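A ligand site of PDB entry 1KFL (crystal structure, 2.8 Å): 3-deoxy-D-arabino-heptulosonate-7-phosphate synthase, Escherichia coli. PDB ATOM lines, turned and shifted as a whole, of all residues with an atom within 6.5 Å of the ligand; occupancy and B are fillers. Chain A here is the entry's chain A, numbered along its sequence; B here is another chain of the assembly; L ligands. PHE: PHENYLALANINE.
N of the ligand is in salt-bridge range of OD1 of Asp 6 of chain B (3.1 Å). The side-chain amide oxygen (OE1) of Gln 151 is in hydrogen-bond range of a nitrogen (N) of the ligand (3.3 Å). N of Asp 7 of chain B is in hydrogen-bond range of OXT of the ligand (3.0 Å). The side-chain carboxylate (OD1) of Asp 7 of chain B is in salt-bridge range of a nitrogen (N) of the ligand, at 2.9 Å. The side-chain amino group (NZ) of Lys 214 lies close to a nitrogen (N) of the ligand (3.2 Å). N of Ser 180 lies within hydrogen-bond range of O of the ligand, at 2.7 Å. The side-chain hydroxyl of Ser 180 is in hydrogen-bond range of an oxygen (OXT) of the ligand, at 2.6 Å.
OG of Ser 180 sits at hydrogen-bond distance from N of Leu 8 of chain B (2.7 Å). OD2 of Asp 7 of chain B is in salt-bridge range of NZ of Lys 214 (3.6 Å). The backbone carbonyl oxygen of Val 212 sits at hydrogen-bond distance from the side-chain amide nitrogen of Gln 151 (2.6 Å). The side-chain carboxylate of Asp 6 of chain B is in salt-bridge range of the side-chain amino group of Lys 214. The backbone carbonyl oxygen (O) of Phe 209 lies within hydrogen-bond range of the backbone NH (N) of Val 221. The guanidinium group of Arg 9 of chain B sits at hydrogen-bond distance from the backbone carbonyl oxygen of Leu 179, at 2.7 Å. OE1 of Gln 151 is in hydrogen-bond range of NZ of Lys 214. The backbone carbonyl oxygen (O) of Ala 154 lies within hydrogen-bond range of the guanidinium group (NH2) of Arg 40 (2.8 Å).
Met 147 touches the ligand (O to CE2, 3.6 Å). Pro 150 touches the ligand (CB to CD2, 3.8 Å). Ala 154 touches the ligand. O of Gly 178 touches CB of the ligand, at 3.8 Å. Leu 179 touches the ligand. Phe 209 touches the ligand. OG of Ser 211 touches CZ of the ligand, at 3.4 Å. Val 221 touches the ligand. Ile 10 of chain B touches the ligand. Along chain A the residues within 4 Å of the ligand span positions 147 to 221. The nearest printed residue that does not touch the ligand is Asn 5 of chain B (4.1 Å).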
ATOM      1  N   ARG A  40     -28.277 -32.743  16.585  1.00  0.00           N
ATOM      2  CA  ARG A  40     -27.046 -33.029  17.324  1.00  0.00           C
ATOM      3  C   ARG A  40     -26.627 -34.440  16.965  1.00  0.00           C
ATOM      4  O   ARG A  40     -25.447 -34.709  16.767  1.00  0.00           O
ATOM      5  CB  ARG A  40     -27.268 -32.940  18.827  1.00  0.00           C
ATOM      6  CG  ARG A  40     -27.497 -31.540  19.367  1.00  0.00           C
ATOM      7  CD  ARG A  40     -27.690 -31.559  20.872  1.00  0.00           C
ATOM      8  NE  ARG A  40     -27.823 -30.206  21.411  1.00  0.00           N
ATOM      9  CZ  ARG A  40     -27.984 -29.929  22.697  1.00  0.00           C
ATOM     10  NH1 ARG A  40     -28.013 -30.914  23.590  1.00  0.00           N
ATOM     11  NH2 ARG A  40     -28.121 -28.679  23.098  1.00  0.00           N
ATOM     12  N   PHE A 144     -20.415 -19.050  21.957  1.00  0.00           N
ATOM     13  CA  PHE A 144     -20.527 -18.837  23.393  1.00  0.00           C
ATOM     14  C   PHE A 144     -19.309 -18.041  23.782  1.00  0.00           C
ATOM     15  O   PHE A 144     -18.185 -18.528  23.674  1.00  0.00           O
ATOM     16  CB  PHE A 144     -20.573 -20.188  24.129  1.00  0.00           C
ATOM     17  CG  PHE A 144     -21.918 -20.888  24.024  1.00  0.00           C
ATOM     18  CD1 PHE A 144     -22.017 -22.183  23.516  1.00  0.00           C
ATOM     19  CD2 PHE A 144     -23.090 -20.219  24.416  1.00  0.00           C
ATOM     20  CE1 PHE A 144     -23.275 -22.822  23.376  1.00  0.00           C
ATOM     21  CE2 PHE A 144     -24.352 -20.841  24.289  1.00  0.00           C
ATOM     22  CZ  PHE A 144     -24.448 -22.152  23.757  1.00  0.00           C
ATOM     23  N   MET A 147     -19.072 -18.129  30.169  1.00  0.00           N
ATOM     24  CA  MET A 147     -19.522 -19.368  30.779  1.00  0.00           C
ATOM     25  C   MET A 147     -20.936 -19.334  31.378  1.00  0.00           C
ATOM     26  O   MET A 147     -21.426 -20.348  31.894  1.00  0.00           O
ATOM     27  CB  MET A 147     -18.514 -19.780  31.853  1.00  0.00           C
ATOM     28  CG  MET A 147     -17.222 -20.435  31.317  1.00  0.00           C
ATOM     29  SD  MET A 147     -16.394 -19.546  29.773  1.00  0.00           S
ATOM     30  CE  MET A 147     -15.635 -18.034  30.730  1.00  0.00           C
ATOM     31  N   ILE A 148     -21.598 -18.186  31.293  1.00  0.00           N
ATOM     32  CA  ILE A 148     -22.910 -18.032  31.905  1.00  0.00           C
ATOM     33  C   ILE A 148     -24.059 -18.052  30.933  1.00  0.00           C
ATOM     34  O   ILE A 148     -25.141 -18.568  31.219  1.00  0.00           O
ATOM     35  CB  ILE A 148     -22.967 -16.723  32.707  1.00  0.00           C
ATOM     36  CG1 ILE A 148     -21.977 -16.799  33.874  1.00  0.00           C
ATOM     37  CG2 ILE A 148     -24.393 -16.454  33.201  1.00  0.00           C
ATOM     38  CD1 ILE A 148     -21.896 -15.541  34.702  1.00  0.00           C
ATOM     39  N   PRO A 150     -24.466 -19.829  28.289  1.00  0.00           N
ATOM     40  CA  PRO A 150     -24.903 -21.176  27.930  1.00  0.00           C
ATOM     41  C   PRO A 150     -26.119 -21.643  28.716  1.00  0.00           C
ATOM     42  O   PRO A 150     -27.038 -22.243  28.130  1.00  0.00           O
ATOM     43  CB  PRO A 150     -23.695 -22.042  28.215  1.00  0.00           C
ATOM     44  CG  PRO A 150     -22.542 -21.100  27.941  1.00  0.00           C
ATOM     45  CD  PRO A 150     -23.012 -19.800  28.569  1.00  0.00           C
ATOM     46  N   GLN A 151     -26.153 -21.335  30.021  1.00  0.00           N
ATOM     47  CA  GLN A 151     -27.255 -21.763  30.878  1.00  0.00           C
ATOM     48  C   GLN A 151     -28.615 -21.300  30.376  1.00  0.00           C
ATOM     49  O   GLN A 151     -29.599 -21.986  30.580  1.00  0.00           O
ATOM     50  CB  GLN A 151     -27.029 -21.302  32.316  1.00  0.00           C
ATOM     51  CG  GLN A 151     -25.954 -22.085  33.076  1.00  0.00           C
ATOM     52  CD  GLN A 151     -26.373 -23.520  33.402  1.00  0.00           C
ATOM     53  OE1 GLN A 151     -26.966 -24.222  32.572  1.00  0.00           O
ATOM     54  NE2 GLN A 151     -26.072 -23.958  34.627  1.00  0.00           N
ATOM     55  N   ALA A 154     -28.093 -22.880  25.661  1.00  0.00           N
ATOM     56  CA  ALA A 154     -27.504 -24.116  25.149  1.00  0.00           C
ATOM     57  C   ALA A 154     -28.498 -25.201  24.776  1.00  0.00           C
ATOM     58  O   ALA A 154     -28.256 -25.967  23.846  1.00  0.00           O
ATOM     59  CB  ALA A 154     -26.522 -24.665  26.122  1.00  0.00           C
ATOM     60  N   ASP A 155     -29.636 -25.267  25.478  1.00  0.00           N
ATOM     61  CA  ASP A 155     -30.597 -26.322  25.169  1.00  0.00           C
ATOM     62  C   ASP A 155     -31.304 -26.112  23.837  1.00  0.00           C
ATOM     63  O   ASP A 155     -32.080 -26.970  23.397  1.00  0.00           O
ATOM     64  CB  ASP A 155     -31.627 -26.471  26.288  1.00  0.00           C
ATOM     65  CG  ASP A 155     -32.480 -25.223  26.490  1.00  0.00           C
ATOM     66  OD1 ASP A 155     -31.937 -24.155  26.872  1.00  0.00           O
ATOM     67  OD2 ASP A 155     -33.706 -25.328  26.279  1.00  0.00           O
ATOM     68  N   LEU A 175     -15.353 -25.037  29.406  1.00  0.00           N
ATOM     69  CA  LEU A 175     -16.766 -24.834  29.058  1.00  0.00           C
ATOM     70  C   LEU A 175     -17.197 -25.721  27.899  1.00  0.00           C
ATOM     71  O   LEU A 175     -18.286 -26.290  27.923  1.00  0.00           O
ATOM     72  CB  LEU A 175     -17.017 -23.371  28.687  1.00  0.00           C
ATOM     73  CG  LEU A 175     -18.257 -23.056  27.822  1.00  0.00           C
ATOM     74  CD1 LEU A 175     -19.530 -23.581  28.480  1.00  0.00           C
ATOM     75  CD2 LEU A 175     -18.349 -21.526  27.616  1.00  0.00           C
ATOM     76  N   GLY A 178     -18.104 -29.224  28.456  1.00  0.00           N
ATOM     77  CA  GLY A 178     -19.365 -29.449  29.160  1.00  0.00           C
ATOM     78  C   GLY A 178     -20.615 -29.172  28.319  1.00  0.00           C
ATOM     79  O   GLY A 178     -21.734 -29.508  28.726  1.00  0.00           O
ATOM     80  N   LEU A 179     -20.456 -28.557  27.150  1.00  0.00           N
ATOM     81  CA  LEU A 179     -21.637 -28.267  26.339  1.00  0.00           C
ATOM     82  C   LEU A 179     -22.304 -29.532  25.812  1.00  0.00           C
ATOM     83  O   LEU A 179     -21.656 -30.522  25.497  1.00  0.00           O
ATOM     84  CB  LEU A 179     -21.292 -27.340  25.169  1.00  0.00           C
ATOM     85  CG  LEU A 179     -20.728 -26.000  25.653  1.00  0.00           C
ATOM     86  CD1 LEU A 179     -20.225 -25.165  24.471  1.00  0.00           C
ATOM     87  CD2 LEU A 179     -21.838 -25.285  26.433  1.00  0.00           C
ATOM     88  N   SER A 180     -23.613 -29.478  25.710  1.00  0.00           N
ATOM     89  CA  SER A 180     -24.361 -30.633  25.263  1.00  0.00           C
ATOM     90  C   SER A 180     -24.422 -30.746  23.770  1.00  0.00           C
ATOM     91  O   SER A 180     -25.142 -31.586  23.249  1.00  0.00           O
ATOM     92  CB  SER A 180     -25.787 -30.557  25.849  1.00  0.00           C
ATOM     93  OG  SER A 180     -25.726 -30.598  27.268  1.00  0.00           O
ATOM     94  N   CYS A 181     -23.655 -29.920  23.071  1.00  0.00           N
ATOM     95  CA  CYS A 181     -23.680 -29.934  21.601  1.00  0.00           C
ATOM     96  C   CYS A 181     -22.271 -29.950  21.005  1.00  0.00           C
ATOM     97  O   CYS A 181     -21.306 -29.560  21.668  1.00  0.00           O
ATOM     98  CB  CYS A 181     -24.382 -28.685  21.097  1.00  0.00           C
ATOM     99  SG  CYS A 181     -23.425 -27.192  21.545  1.00  0.00           S
ATOM    100  N   PHE A 209     -15.291 -25.700  36.006  1.00  0.00           N
ATOM    101  CA  PHE A 209     -15.304 -24.270  35.710  1.00  0.00           C
ATOM    102  C   PHE A 209     -16.468 -23.663  36.487  1.00  0.00           C
ATOM    103  O   PHE A 209     -17.425 -24.370  36.798  1.00  0.00           O
ATOM    104  CB  PHE A 209     -15.382 -23.978  34.209  1.00  0.00           C
ATOM    105  CG  PHE A 209     -16.690 -24.327  33.569  1.00  0.00           C
ATOM    106  CD1 PHE A 209     -17.741 -23.423  33.565  1.00  0.00           C
ATOM    107  CD2 PHE A 209     -16.866 -25.570  32.940  1.00  0.00           C
ATOM    108  CE1 PHE A 209     -18.951 -23.750  32.944  1.00  0.00           C
ATOM    109  CE2 PHE A 209     -18.074 -25.906  32.318  1.00  0.00           C
ATOM    110  CZ  PHE A 209     -19.118 -24.990  32.316  1.00  0.00           C
ATOM    111  N   LEU A 210     -16.362 -22.395  36.849  1.00  0.00           N
ATOM    112  CA  LEU A 210     -17.405 -21.735  37.628  1.00  0.00           C
ATOM    113  C   LEU A 210     -18.405 -21.119  36.666  1.00  0.00           C
ATOM    114  O   LEU A 210     -18.054 -20.755  35.551  1.00  0.00           O
ATOM    115  CB  LEU A 210     -16.821 -20.653  38.557  1.00  0.00           C
ATOM    116  CG  LEU A 210     -15.625 -21.152  39.386  1.00  0.00           C
ATOM    117  CD1 LEU A 210     -15.116 -20.098  40.365  1.00  0.00           C
ATOM    118  CD2 LEU A 210     -16.035 -22.383  40.137  1.00  0.00           C
ATOM    119  N   SER A 211     -19.665 -21.046  37.091  1.00  0.00           N
ATOM    120  CA  SER A 211     -20.748 -20.502  36.305  1.00  0.00           C
ATOM    121  C   SER A 211     -21.939 -20.404  37.257  1.00  0.00           C
ATOM    122  O   SER A 211     -21.763 -20.070  38.435  1.00  0.00           O
ATOM    123  CB  SER A 211     -21.057 -21.418  35.135  1.00  0.00           C
ATOM    124  OG  SER A 211     -22.246 -20.978  34.479  1.00  0.00           O
ATOM    125  N   VAL A 212     -23.151 -20.683  36.796  1.00  0.00           N
ATOM    126  CA  VAL A 212     -24.282 -20.615  37.710  1.00  0.00           C
ATOM    127  C   VAL A 212     -25.286 -21.737  37.545  1.00  0.00           C
ATOM    128  O   VAL A 212     -25.511 -22.232  36.436  1.00  0.00           O
ATOM    129  CB  VAL A 212     -25.049 -19.269  37.589  1.00  0.00           C
ATOM    130  CG1 VAL A 212     -24.094 -18.119  37.822  1.00  0.00           C
ATOM    131  CG2 VAL A 212     -25.750 -19.158  36.232  1.00  0.00           C
ATOM    132  N   LYS A 214     -28.992 -23.516  37.406  1.00  0.00           N
ATOM    133  CA  LYS A 214     -30.140 -23.075  36.626  1.00  0.00           C
ATOM    134  C   LYS A 214     -30.947 -22.061  37.418  1.00  0.00           C
ATOM    135  O   LYS A 214     -31.737 -21.296  36.844  1.00  0.00           O
ATOM    136  CB  LYS A 214     -31.024 -24.262  36.283  1.00  0.00           C
ATOM    137  CG  LYS A 214     -31.225 -24.469  34.812  1.00  0.00           C
ATOM    138  CD  LYS A 214     -29.926 -24.847  34.136  1.00  0.00           C
ATOM    139  CE  LYS A 214     -30.172 -25.349  32.723  1.00  0.00           C
ATOM    140  NZ  LYS A 214     -28.938 -26.059  32.302  1.00  0.00           N
ATOM    141  N   VAL A 221     -18.993 -26.213  38.097  1.00  0.00           N
ATOM    142  CA  VAL A 221     -19.450 -27.229  37.163  1.00  0.00           C
ATOM    143  C   VAL A 221     -18.389 -28.252  36.894  1.00  0.00           C
ATOM    144  O   VAL A 221     -17.230 -27.907  36.690  1.00  0.00           O
ATOM    145  CB  VAL A 221     -19.847 -26.629  35.815  1.00  0.00           C
ATOM    146  CG1 VAL A 221     -20.374 -27.729  34.901  1.00  0.00           C
ATOM    147  CG2 VAL A 221     -20.915 -25.582  35.997  1.00  0.00           C
ATOM    148  N   ASN B   5     -32.860 -31.891  26.373  1.00  0.00           N
ATOM    149  CA  ASN B   5     -31.581 -31.578  25.733  1.00  0.00           C
ATOM    150  C   ASN B   5     -30.639 -30.788  26.661  1.00  0.00           C
ATOM    151  O   ASN B   5     -29.692 -30.122  26.202  1.00  0.00           O
ATOM    152  CB  ASN B   5     -31.811 -30.791  24.417  1.00  0.00           C
ATOM    153  CG  ASN B   5     -32.769 -31.524  23.438  1.00  0.00           C
ATOM    154  OD1 ASN B   5     -32.597 -32.709  23.146  1.00  0.00           O
ATOM    155  ND2 ASN B   5     -33.758 -30.788  22.899  1.00  0.00           N
ATOM    156  N   ASP B   6     -30.878 -30.870  27.966  1.00  0.00           N
ATOM    157  CA  ASP B   6     -30.064 -30.106  28.906  1.00  0.00           C
ATOM    158  C   ASP B   6     -28.981 -30.882  29.647  1.00  0.00           C
ATOM    159  O   ASP B   6     -29.079 -32.087  29.861  1.00  0.00           O
ATOM    160  CB  ASP B   6     -30.978 -29.418  29.916  1.00  0.00           C
ATOM    161  CG  ASP B   6     -30.240 -28.448  30.821  1.00  0.00           C
ATOM    162  OD1 ASP B   6     -29.464 -27.610  30.315  1.00  0.00           O
ATOM    163  OD2 ASP B   6     -30.449 -28.531  32.054  1.00  0.00           O
ATOM    164  N   ASP B   7     -27.925 -30.177  30.010  1.00  0.00           N
ATOM    165  CA  ASP B   7     -26.796 -30.739  30.731  1.00  0.00           C
ATOM    166  C   ASP B   7     -26.279 -32.129  30.340  1.00  0.00           C
ATOM    167  O   ASP B   7     -25.704 -32.826  31.168  1.00  0.00           O
ATOM    168  CB  ASP B   7     -27.083 -30.721  32.236  1.00  0.00           C
ATOM    169  CG  ASP B   7     -26.974 -29.303  32.844  1.00  0.00           C
ATOM    170  OD1 ASP B   7     -26.203 -28.484  32.316  1.00  0.00           O
ATOM    171  OD2 ASP B   7     -27.659 -29.005  33.854  1.00  0.00           O
ATOM    172  N   LEU B   8     -26.419 -32.523  29.081  1.00  0.00           N
ATOM    173  CA  LEU B   8     -25.934 -33.834  28.664  1.00  0.00           C
ATOM    174  C   LEU B   8     -24.487 -34.160  29.051  1.00  0.00           C
ATOM    175  O   LEU B   8     -24.172 -35.326  29.191  1.00  0.00           O
ATOM    176  CB  LEU B   8     -26.076 -34.030  27.161  1.00  0.00           C
ATOM    177  CG  LEU B   8     -27.476 -33.767  26.600  1.00  0.00           C
ATOM    178  CD1 LEU B   8     -27.560 -34.219  25.146  1.00  0.00           C
ATOM    179  CD2 LEU B   8     -28.485 -34.502  27.436  1.00  0.00           C
ATOM    180  N   ARG B   9     -23.614 -33.167  29.214  1.00  0.00           N
ATOM    181  CA  ARG B   9     -22.220 -33.491  29.564  1.00  0.00           C
ATOM    182  C   ARG B   9     -21.787 -32.993  30.926  1.00  0.00           C
ATOM    183  O   ARG B   9     -20.595 -32.799  31.173  1.00  0.00           O
ATOM    184  CB  ARG B   9     -21.224 -32.946  28.527  1.00  0.00           C
ATOM    185  CG  ARG B   9     -21.332 -33.574  27.149  1.00  0.00           C
ATOM    186  CD  ARG B   9     -20.113 -33.234  26.252  1.00  0.00           C
ATOM    187  NE  ARG B   9     -20.173 -34.079  25.061  1.00  0.00           N
ATOM    188  CZ  ARG B   9     -20.919 -33.828  23.991  1.00  0.00           C
ATOM    189  NH1 ARG B   9     -21.666 -32.710  23.945  1.00  0.00           N
ATOM    190  NH2 ARG B   9     -21.011 -34.739  23.014  1.00  0.00           N
ATOM    191  N   ILE B  10     -22.751 -32.780  31.805  1.00  0.00           N
ATOM    192  CA  ILE B  10     -22.434 -32.310  33.149  1.00  0.00           C
ATOM    193  C   ILE B  10     -22.449 -33.465  34.137  1.00  0.00           C
ATOM    194  O   ILE B  10     -23.495 -34.036  34.432  1.00  0.00           O
ATOM    195  CB  ILE B  10     -23.446 -31.271  33.650  1.00  0.00           C
ATOM    196  CG1 ILE B  10     -23.543 -30.124  32.657  1.00  0.00           C
ATOM    197  CG2 ILE B  10     -22.983 -30.731  34.998  1.00  0.00           C
ATOM    198  CD1 ILE B  10     -22.215 -29.407  32.441  1.00  0.00           C
ATOM    199  N   ILE B  13     -23.069 -30.473  39.164  1.00  0.00           N
ATOM    200  CA  ILE B  13     -22.981 -29.028  39.382  1.00  0.00           C
ATOM    201  C   ILE B  13     -23.535 -28.672  40.760  1.00  0.00           C
ATOM    202  O   ILE B  13     -24.681 -28.945  41.056  1.00  0.00           O
ATOM    203  CB  ILE B  13     -23.775 -28.254  38.303  1.00  0.00           C
ATOM    204  CG1 ILE B  13     -23.858 -26.785  38.665  1.00  0.00           C
ATOM    205  CG2 ILE B  13     -25.144 -28.789  38.174  1.00  0.00           C
ATOM    206  CD1 ILE B  13     -24.497 -25.975  37.564  1.00  0.00           C
HETATM  207  N   PHE L   1     -26.522 -26.539  30.199  1.00  0.00           N
HETATM  208  CA  PHE L   1     -25.425 -26.518  29.259  1.00  0.00           C
HETATM  209  C   PHE L   1     -25.625 -27.493  28.116  1.00  0.00           C
HETATM  210  O   PHE L   1     -24.765 -27.514  27.171  1.00  0.00           O
HETATM  211  CB  PHE L   1     -24.096 -26.783  29.966  1.00  0.00           C
HETATM  212  CG  PHE L   1     -23.611 -25.868  31.046  1.00  0.00           C
HETATM  213  CD1 PHE L   1     -23.904 -26.019  32.424  1.00  0.00           C
HETATM  214  CD2 PHE L   1     -22.777 -24.783  30.657  1.00  0.00           C
HETATM  215  CE1 PHE L   1     -23.375 -25.080  33.364  1.00  0.00           C
HETATM  216  CE2 PHE L   1     -22.237 -23.845  31.566  1.00  0.00           C
HETATM  217  CZ  PHE L   1     -22.540 -23.999  32.944  1.00  0.00           C
HETATM  218  OXT PHE L   1     -26.616 -28.273  28.114  1.00  0.00           O
